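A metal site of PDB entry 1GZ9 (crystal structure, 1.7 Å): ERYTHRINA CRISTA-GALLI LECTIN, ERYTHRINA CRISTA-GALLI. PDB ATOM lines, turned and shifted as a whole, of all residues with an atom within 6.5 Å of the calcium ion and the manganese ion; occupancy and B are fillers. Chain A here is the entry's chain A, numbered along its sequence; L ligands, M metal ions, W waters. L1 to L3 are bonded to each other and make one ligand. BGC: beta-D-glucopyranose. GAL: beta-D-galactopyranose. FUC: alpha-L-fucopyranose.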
ATOM      1  N   ASP A  89     -15.346 -26.538   8.900  1.00  0.00           N
ATOM      2  CA  ASP A  89     -15.122 -25.181   8.383  1.00  0.00           C
ATOM      3  C   ASP A  89     -13.618 -24.780   8.388  1.00  0.00           C
ATOM      4  O   ASP A  89     -13.211 -23.919   7.597  1.00  0.00           O
ATOM      5  CB  ASP A  89     -15.896 -24.179   9.231  1.00  0.00           C
ATOM      6  CG  ASP A  89     -17.266 -23.818   8.640  1.00  0.00           C
ATOM      7  OD1 ASP A  89     -17.319 -23.085   7.619  1.00  0.00           O
ATOM      8  OD2 ASP A  89     -18.300 -24.275   9.203  1.00  0.00           O
ATOM      9  N   GLY A 107     -18.197 -20.877   9.807  1.00  0.00           N
ATOM     10  CA  GLY A 107     -17.192 -20.149   9.049  1.00  0.00           C
ATOM     11  C   GLY A 107     -16.485 -19.031   9.830  1.00  0.00           C
ATOM     12  O   GLY A 107     -15.483 -18.466   9.341  1.00  0.00           O
ATOM     13  N   TYR A 108     -16.959 -18.713  11.023  1.00  0.00           N
ATOM     14  CA  TYR A 108     -16.323 -17.666  11.820  1.00  0.00           C
ATOM     15  C   TYR A 108     -15.202 -18.232  12.683  1.00  0.00           C
ATOM     16  O   TYR A 108     -14.498 -17.481  13.389  1.00  0.00           O
ATOM     17  CB  TYR A 108     -17.356 -16.943  12.679  1.00  0.00           C
ATOM     18  CG  TYR A 108     -18.482 -16.399  11.816  1.00  0.00           C
ATOM     19  CD1 TYR A 108     -18.306 -15.267  11.030  1.00  0.00           C
ATOM     20  CD2 TYR A 108     -19.720 -17.080  11.733  1.00  0.00           C
ATOM     21  CE1 TYR A 108     -19.318 -14.806  10.176  1.00  0.00           C
ATOM     22  CE2 TYR A 108     -20.737 -16.626  10.879  1.00  0.00           C
ATOM     23  CZ  TYR A 108     -20.517 -15.491  10.109  1.00  0.00           C
ATOM     24  OH  TYR A 108     -21.492 -15.076   9.220  1.00  0.00           O
ATOM     25  N   LEU A 109     -15.057 -19.545  12.593  1.00  0.00           N
ATOM     26  CA  LEU A 109     -13.996 -20.324  13.218  1.00  0.00           C
ATOM     27  C   LEU A 109     -13.791 -20.187  14.727  1.00  0.00           C
ATOM     28  O   LEU A 109     -12.702 -20.514  15.234  1.00  0.00           O
ATOM     29  CB  LEU A 109     -12.676 -20.016  12.455  1.00  0.00           C
ATOM     30  CG  LEU A 109     -12.734 -20.160  10.912  1.00  0.00           C
ATOM     31  CD1 LEU A 109     -11.331 -19.861  10.262  1.00  0.00           C
ATOM     32  CD2 LEU A 109     -13.086 -21.611  10.566  1.00  0.00           C
ATOM     33  N   GLU A 127      -5.616 -18.499   9.313  1.00  0.00           N
ATOM     34  CA  GLU A 127      -6.601 -19.567   9.111  1.00  0.00           C
ATOM     35  C   GLU A 127      -6.216 -20.584   8.058  1.00  0.00           C
ATOM     36  O   GLU A 127      -5.411 -20.284   7.183  1.00  0.00           O
ATOM     37  CB  GLU A 127      -7.927 -18.930   8.720  1.00  0.00           C
ATOM     38  CG  GLU A 127      -7.890 -18.189   7.369  1.00  0.00           C
ATOM     39  CD  GLU A 127      -9.265 -17.767   6.860  1.00  0.00           C
ATOM     40  OE1 GLU A 127     -10.069 -17.149   7.626  1.00  0.00           O
ATOM     41  OE2 GLU A 127      -9.485 -18.053   5.672  1.00  0.00           O
ATOM     42  N   ASP A 129      -8.630 -22.601   6.060  1.00  0.00           N
ATOM     43  CA  ASP A 129     -10.093 -22.596   5.815  1.00  0.00           C
ATOM     44  C   ASP A 129     -10.506 -23.598   4.777  1.00  0.00           C
ATOM     45  O   ASP A 129      -9.975 -23.593   3.663  1.00  0.00           O
ATOM     46  CB  ASP A 129     -10.428 -21.146   5.371  1.00  0.00           C
ATOM     47  CG  ASP A 129     -11.918 -20.862   5.253  1.00  0.00           C
ATOM     48  OD1 ASP A 129     -12.714 -21.799   5.306  1.00  0.00           O
ATOM     49  OD2 ASP A 129     -12.254 -19.667   5.088  1.00  0.00           O
ATOM     50  N   THR A 130     -11.475 -24.449   5.128  1.00  0.00           N
ATOM     51  CA  THR A 130     -11.907 -25.527   4.272  1.00  0.00           C
ATOM     52  C   THR A 130     -13.247 -25.367   3.575  1.00  0.00           C
ATOM     53  O   THR A 130     -13.607 -26.228   2.785  1.00  0.00           O
ATOM     54  CB  THR A 130     -11.979 -26.849   5.066  1.00  0.00           C
ATOM     55  OG1 THR A 130     -12.791 -26.630   6.220  1.00  0.00           O
ATOM     56  CG2 THR A 130     -10.600 -27.277   5.535  1.00  0.00           C
ATOM     57  N   PHE A 131     -13.970 -24.264   3.837  1.00  0.00           N
ATOM     58  CA  PHE A 131     -15.299 -24.084   3.210  1.00  0.00           C
ATOM     59  C   PHE A 131     -15.394 -22.683   2.683  1.00  0.00           C
ATOM     60  O   PHE A 131     -15.153 -21.726   3.436  1.00  0.00           O
ATOM     61  CB  PHE A 131     -16.401 -24.307   4.255  1.00  0.00           C
ATOM     62  CG  PHE A 131     -17.812 -24.107   3.686  1.00  0.00           C
ATOM     63  CD1 PHE A 131     -18.510 -25.165   3.136  1.00  0.00           C
ATOM     64  CD2 PHE A 131     -18.389 -22.829   3.695  1.00  0.00           C
ATOM     65  CE1 PHE A 131     -19.799 -24.960   2.576  1.00  0.00           C
ATOM     66  CE2 PHE A 131     -19.671 -22.618   3.134  1.00  0.00           C
ATOM     67  CZ  PHE A 131     -20.370 -23.676   2.574  1.00  0.00           C
ATOM     68  N   SER A 132     -15.822 -22.539   1.429  1.00  0.00           N
ATOM     69  CA  SER A 132     -15.892 -21.190   0.809  1.00  0.00           C
ATOM     70  C   SER A 132     -17.206 -20.475   1.172  1.00  0.00           C
ATOM     71  O   SER A 132     -18.276 -20.755   0.585  1.00  0.00           O
ATOM     72  CB  SER A 132     -15.796 -21.293  -0.718  1.00  0.00           C
ATOM     73  OG  SER A 132     -15.651 -20.005  -1.298  1.00  0.00           O
ATOM     74  N   ASN A 133     -17.109 -19.591   2.147  1.00  0.00           N
ATOM     75  CA  ASN A 133     -18.260 -18.771   2.596  1.00  0.00           C
ATOM     76  C   ASN A 133     -18.450 -17.582   1.614  1.00  0.00           C
ATOM     77  O   ASN A 133     -17.610 -17.335   0.755  1.00  0.00           O
ATOM     78  CB  ASN A 133     -17.960 -18.212   3.991  1.00  0.00           C
ATOM     79  CG  ASN A 133     -17.965 -19.298   5.043  1.00  0.00           C
ATOM     80  OD1 ASN A 133     -16.935 -19.917   5.341  1.00  0.00           O
ATOM     81  ND2 ASN A 133     -19.158 -19.584   5.593  1.00  0.00           N
ATOM     82  N   TRP A 135     -17.778 -14.567   1.838  1.00  0.00           N
ATOM     83  CA  TRP A 135     -16.695 -13.601   1.909  1.00  0.00           C
ATOM     84  C   TRP A 135     -15.342 -14.221   1.534  1.00  0.00           C
ATOM     85  O   TRP A 135     -14.301 -13.521   1.586  1.00  0.00           O
ATOM     86  CB  TRP A 135     -16.553 -13.064   3.349  1.00  0.00           C
ATOM     87  CG  TRP A 135     -16.342 -14.216   4.370  1.00  0.00           C
ATOM     88  CD1 TRP A 135     -15.159 -14.885   4.643  1.00  0.00           C
ATOM     89  CD2 TRP A 135     -17.345 -14.824   5.190  1.00  0.00           C
ATOM     90  NE1 TRP A 135     -15.375 -15.882   5.586  1.00  0.00           N
ATOM     91  CE2 TRP A 135     -16.706 -15.856   5.941  1.00  0.00           C
ATOM     92  CE3 TRP A 135     -18.725 -14.601   5.372  1.00  0.00           C
ATOM     93  CZ2 TRP A 135     -17.414 -16.653   6.852  1.00  0.00           C
ATOM     94  CZ3 TRP A 135     -19.419 -15.396   6.271  1.00  0.00           C
ATOM     95  CH2 TRP A 135     -18.745 -16.417   7.019  1.00  0.00           C
ATOM     96  N   ASP A 136     -15.359 -15.508   1.189  1.00  0.00           N
ATOM     97  CA  ASP A 136     -14.119 -16.238   0.864  1.00  0.00           C
ATOM     98  C   ASP A 136     -13.759 -16.347  -0.598  1.00  0.00           C
ATOM     99  O   ASP A 136     -14.601 -16.197  -1.461  1.00  0.00           O
ATOM    100  CB  ASP A 136     -14.238 -17.726   1.299  1.00  0.00           C
ATOM    101  CG  ASP A 136     -13.967 -17.946   2.788  1.00  0.00           C
ATOM    102  OD1 ASP A 136     -13.009 -17.368   3.298  1.00  0.00           O
ATOM    103  OD2 ASP A 136     -14.717 -18.713   3.421  1.00  0.00           O
ATOM    104  N   PRO A 137     -12.477 -16.641  -0.892  1.00  0.00           N
ATOM    105  CA  PRO A 137     -12.053 -16.825  -2.269  1.00  0.00           C
ATOM    106  C   PRO A 137     -12.665 -18.186  -2.560  1.00  0.00           C
ATOM    107  O   PRO A 137     -13.004 -18.937  -1.633  1.00  0.00           O
ATOM    108  CB  PRO A 137     -10.532 -16.914  -2.172  1.00  0.00           C
ATOM    109  CG  PRO A 137     -10.296 -17.369  -0.753  1.00  0.00           C
ATOM    110  CD  PRO A 137     -11.305 -16.543   0.004  1.00  0.00           C
ATOM    111  N   VAL A 140     -10.720 -23.878  -1.976  1.00  0.00           N
ATOM    112  CA  VAL A 140     -10.552 -24.359  -0.622  1.00  0.00           C
ATOM    113  C   VAL A 140      -9.892 -25.712  -0.720  1.00  0.00           C
ATOM    114  O   VAL A 140     -10.098 -26.463  -1.674  1.00  0.00           O
ATOM    115  CB  VAL A 140     -11.911 -24.515   0.186  1.00  0.00           C
ATOM    116  CG1 VAL A 140     -12.375 -23.131   0.668  1.00  0.00           C
ATOM    117  CG2 VAL A 140     -13.010 -25.196  -0.713  1.00  0.00           C
ATOM    118  N   HIS A 142      -7.766 -22.973   1.857  1.00  0.00           N
ATOM    119  CA  HIS A 142      -6.844 -21.866   1.643  1.00  0.00           C
ATOM    120  C   HIS A 142      -6.262 -21.402   2.990  1.00  0.00           C
ATOM    121  O   HIS A 142      -6.853 -21.582   4.058  1.00  0.00           O
ATOM    122  CB  HIS A 142      -7.505 -20.659   0.896  1.00  0.00           C
ATOM    123  CG  HIS A 142      -8.727 -20.105   1.559  1.00  0.00           C
ATOM    124  ND1 HIS A 142     -10.003 -20.449   1.152  1.00  0.00           N
ATOM    125  CD2 HIS A 142      -8.883 -19.230   2.568  1.00  0.00           C
ATOM    126  CE1 HIS A 142     -10.889 -19.817   1.895  1.00  0.00           C
ATOM    127  NE2 HIS A 142     -10.241 -19.061   2.768  1.00  0.00           N
ATOM    128  N   ILE A 143      -5.055 -20.834   2.945  1.00  0.00           N
ATOM    129  CA  ILE A 143      -4.504 -20.250   4.146  1.00  0.00           C
ATOM    130  C   ILE A 143      -4.982 -18.805   3.997  1.00  0.00           C
ATOM    131  O   ILE A 143      -5.053 -18.298   2.864  1.00  0.00           O
ATOM    132  CB  ILE A 143      -2.971 -20.164   4.074  1.00  0.00           C
ATOM    133  CG1 ILE A 143      -2.402 -21.557   3.803  1.00  0.00           C
ATOM    134  CG2 ILE A 143      -2.427 -19.568   5.366  1.00  0.00           C
ATOM    135  CD1 ILE A 143      -0.849 -21.555   3.708  1.00  0.00           C
ATOM    136  N   GLY A 144      -5.290 -18.187   5.118  1.00  0.00           N
ATOM    137  CA  GLY A 144      -5.659 -16.771   5.109  1.00  0.00           C
ATOM    138  C   GLY A 144      -5.029 -15.994   6.275  1.00  0.00           C
ATOM    139  O   GLY A 144      -4.795 -16.535   7.361  1.00  0.00           O
ATOM    140  N   ASP A 146      -5.888 -12.948   8.551  1.00  0.00           N
ATOM    141  CA  ASP A 146      -7.070 -12.230   9.032  1.00  0.00           C
ATOM    142  C   ASP A 146      -6.696 -11.160  10.024  1.00  0.00           C
ATOM    143  O   ASP A 146      -6.077 -11.439  11.048  1.00  0.00           O
ATOM    144  CB  ASP A 146      -8.059 -13.211   9.725  1.00  0.00           C
ATOM    145  CG  ASP A 146      -8.504 -14.346   8.829  1.00  0.00           C
ATOM    146  OD1 ASP A 146      -8.171 -14.300   7.613  1.00  0.00           O
ATOM    147  OD2 ASP A 146      -9.200 -15.298   9.335  1.00  0.00           O
ATOM    148  N   ILE A 150     -12.906 -11.827   9.522  1.00  0.00           N
ATOM    149  CA  ILE A 150     -12.859 -13.181   8.959  1.00  0.00           C
ATOM    150  C   ILE A 150     -12.613 -13.058   7.420  1.00  0.00           C
ATOM    151  O   ILE A 150     -12.296 -14.046   6.736  1.00  0.00           O
ATOM    152  CB  ILE A 150     -14.211 -13.929   9.197  1.00  0.00           C
ATOM    153  CG1 ILE A 150     -14.061 -15.421   8.833  1.00  0.00           C
ATOM    154  CG2 ILE A 150     -15.312 -13.312   8.363  1.00  0.00           C
ATOM    155  CD1 ILE A 150     -13.058 -16.160   9.725  1.00  0.00           C
ATOM    156  N   ARG A 151     -12.750 -11.845   6.875  1.00  0.00           N
ATOM    157  CA  ARG A 151     -12.511 -11.618   5.439  1.00  0.00           C
ATOM    158  C   ARG A 151     -11.038 -11.316   5.315  1.00  0.00           C
ATOM    159  O   ARG A 151     -10.596 -10.168   5.569  1.00  0.00           O
ATOM    160  CB  ARG A 151     -13.314 -10.421   4.926  1.00  0.00           C
ATOM    161  CG  ARG A 151     -14.810 -10.633   5.114  1.00  0.00           C
ATOM    162  CD  ARG A 151     -15.644  -9.597   4.340  1.00  0.00           C
ATOM    163  NE  ARG A 151     -17.055  -9.769   4.651  1.00  0.00           N
ATOM    164  CZ  ARG A 151     -18.020  -9.870   3.745  1.00  0.00           C
ATOM    165  NH1 ARG A 151     -17.732  -9.805   2.454  1.00  0.00           N
ATOM    166  NH2 ARG A 151     -19.273 -10.116   4.151  1.00  0.00           N
ATOM    167  N   SER A 152     -10.268 -12.326   4.880  1.00  0.00           N
ATOM    168  CA  SER A 152      -8.808 -12.205   4.825  1.00  0.00           C
ATOM    169  C   SER A 152      -8.253 -11.082   3.973  1.00  0.00           C
ATOM    170  O   SER A 152      -8.775 -10.835   2.880  1.00  0.00           O
ATOM    171  CB  SER A 152      -8.209 -13.498   4.282  1.00  0.00           C
ATOM    172  OG  SER A 152      -8.638 -14.601   5.052  1.00  0.00           O
ATOM    173  N   THR A 155      -4.971 -14.431   0.844  1.00  0.00           N
ATOM    174  CA  THR A 155      -5.145 -15.882   0.953  1.00  0.00           C
ATOM    175  C   THR A 155      -4.244 -16.608  -0.023  1.00  0.00           C
ATOM    176  O   THR A 155      -3.744 -16.033  -0.997  1.00  0.00           O
ATOM    177  CB  THR A 155      -6.627 -16.333   0.685  1.00  0.00           C
ATOM    178  OG1 THR A 155      -7.030 -15.887  -0.618  1.00  0.00           O
ATOM    179  CG2 THR A 155      -7.580 -15.705   1.705  1.00  0.00           C
HETATM  180  C2  BGC L   1     -27.619 -24.424   5.874  1.00  0.00           C
HETATM  181  C3  BGC L   1     -26.265 -24.164   6.584  1.00  0.00           C
HETATM  182  C4  BGC L   1     -25.625 -22.869   6.048  1.00  0.00           C
HETATM  183  C5  BGC L   1     -26.583 -21.670   6.172  1.00  0.00           C
HETATM  184  C6  BGC L   1     -26.061 -20.432   5.445  1.00  0.00           C
HETATM  185  C1  BGC L   1     -28.514 -23.194   6.103  1.00  0.00           C
HETATM  186  O1  BGC L   1     -29.730 -23.407   5.461  1.00  0.00           O
HETATM  187  O2  BGC L   1     -28.197 -25.601   6.436  1.00  0.00           O
HETATM  188  O3  BGC L   1     -25.429 -25.280   6.382  1.00  0.00           O
HETATM  189  O4  BGC L   1     -24.414 -22.496   6.853  1.00  0.00           O
HETATM  190  O5  BGC L   1     -27.853 -22.010   5.523  1.00  0.00           O
HETATM  191  O6  BGC L   1     -26.657 -19.246   6.007  1.00  0.00           O
HETATM  192  C1  GAL L   2     -23.090 -22.802   6.304  1.00  0.00           C
HETATM  193  C2  GAL L   2     -22.137 -22.055   7.158  1.00  0.00           C
HETATM  194  C3  GAL L   2     -20.690 -22.442   6.556  1.00  0.00           C
HETATM  195  C4  GAL L   2     -20.495 -23.967   6.650  1.00  0.00           C
HETATM  196  C5  GAL L   2     -21.634 -24.611   5.815  1.00  0.00           C
HETATM  197  C6  GAL L   2     -21.599 -26.099   5.834  1.00  0.00           C
HETATM  198  O2  GAL L   2     -22.438 -20.671   6.931  1.00  0.00           O
HETATM  199  O3  GAL L   2     -19.679 -21.759   7.354  1.00  0.00           O
HETATM  200  O4  GAL L   2     -20.606 -24.451   7.991  1.00  0.00           O
HETATM  201  O5  GAL L   2     -22.909 -24.215   6.361  1.00  0.00           O
HETATM  202  O6  GAL L   2     -22.622 -26.532   4.920  1.00  0.00           O
HETATM  203  C1  FUC L   3     -21.928 -19.598   7.700  1.00  0.00           C
HETATM  204  C2  FUC L   3     -22.267 -18.340   6.863  1.00  0.00           C
HETATM  205  C3  FUC L   3     -23.765 -17.888   6.828  1.00  0.00           C
HETATM  206  C4  FUC L   3     -24.410 -17.973   8.253  1.00  0.00           C
HETATM  207  C5  FUC L   3     -24.156 -19.383   8.865  1.00  0.00           C
HETATM  208  C6  FUC L   3     -24.772 -19.530  10.317  1.00  0.00           C
HETATM  209  O2  FUC L   3     -21.501 -18.291   5.637  1.00  0.00           O
HETATM  210  O3  FUC L   3     -23.807 -16.541   6.366  1.00  0.00           O
HETATM  211  O4  FUC L   3     -23.835 -16.989   9.095  1.00  0.00           O
HETATM  212  O5  FUC L   3     -22.658 -19.674   8.983  1.00  0.00           O
HETATM  213 CA    CA M   1     -14.590 -20.264   5.229  1.00  0.00          CA
HETATM  214 MN    MN M   2     -11.280 -17.837   4.426  1.00  0.00          MN
HETATM  215  O   HOH W   1     -12.218 -16.763   6.274  1.00  0.00           O
HETATM  216  O   HOH W   2     -10.527 -15.923   3.625  1.00  0.00           O
HETATM  217  O   HOH W   3     -15.092 -21.986   6.782  1.00  0.00           O
HETATM  218  O   HOH W   4     -14.253 -18.521   6.855  1.00  0.00           O
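N of Glu 127 lies within hydrogen-bond range of O of Gly 144, at 2.9 Å. The side-chain carboxylate (OE1) of Glu 127 sits close to the side-chain carboxylate (OD2) of Asp 146 (2.7 Å).
Water W4 bridges O of Gly 107 (2.8 Å) and NE1 of Trp 135 (3.1 Å). Water W1 lies within hydrogen-bond range of OE1 of Glu 127 (2.6 Å), O of Ile 150 (2.8 Å) and NE1 of Trp 135 (3.3 Å).
Water W3 is bound to the calcium ion (2.4 Å). The calcium ion is bound by the side-chain amide oxygen (OD1) of Asn 133 (2.4 Å). The backbone carbonyl oxygen (O) of Phe 131 is bound to the calcium ion. OD2 of Asp 136 binds the calcium ion (2.4 Å). The calcium ion is bound by water W4, at 2.4 Å. OD2 of Asp 129 binds the calcium ion. The calcium ion is bound by OD1 of Asp 129 (2.4 Å). The calcium ion has seven donor atoms within binding distance.
Along chain A the residues within 4 Å of the manganese ion span positions 127 to 142.
The side-chain hydroxyl (OH) of Tyr 108 is in hydrogen-bond range of an oxygen (O4) of FUC L3 (3.0 Å). An oxygen (O4) of GAL L2 sits at hydrogen-bond distance from the side-chain carboxylate of Asp 89 (2.6 Å). The backbone NH (N) of Gly 107 is in hydrogen-bond range of an oxygen (O3) of GAL L2, at 3.0 Å. ND2 of Asn 133 lies within hydrogen-bond range of O2 of FUC L3 (2.7 Å).
OD1 of Asp 136 is bound to the manganese ion, 2.1 Å away. OD2 of Asp 129 is bound to the manganese ion (2.2 Å). The manganese ion is bound by OE2 of Glu 127, 2.2 Å away. Water W2 is bound to the manganese ion (2.2 Å). The manganese ion is bound by NE2 of His 142, at 2.3 Å. Water W1 is bound to the manganese ion (2.3 Å). The manganese ion has six donor atoms within binding distance.
Of the 22 residues printed, 4 come within 4 Å of the calcium ion. The nearest printed residue that does not touch the calcium ion is Trp 135 (4.5 Å).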
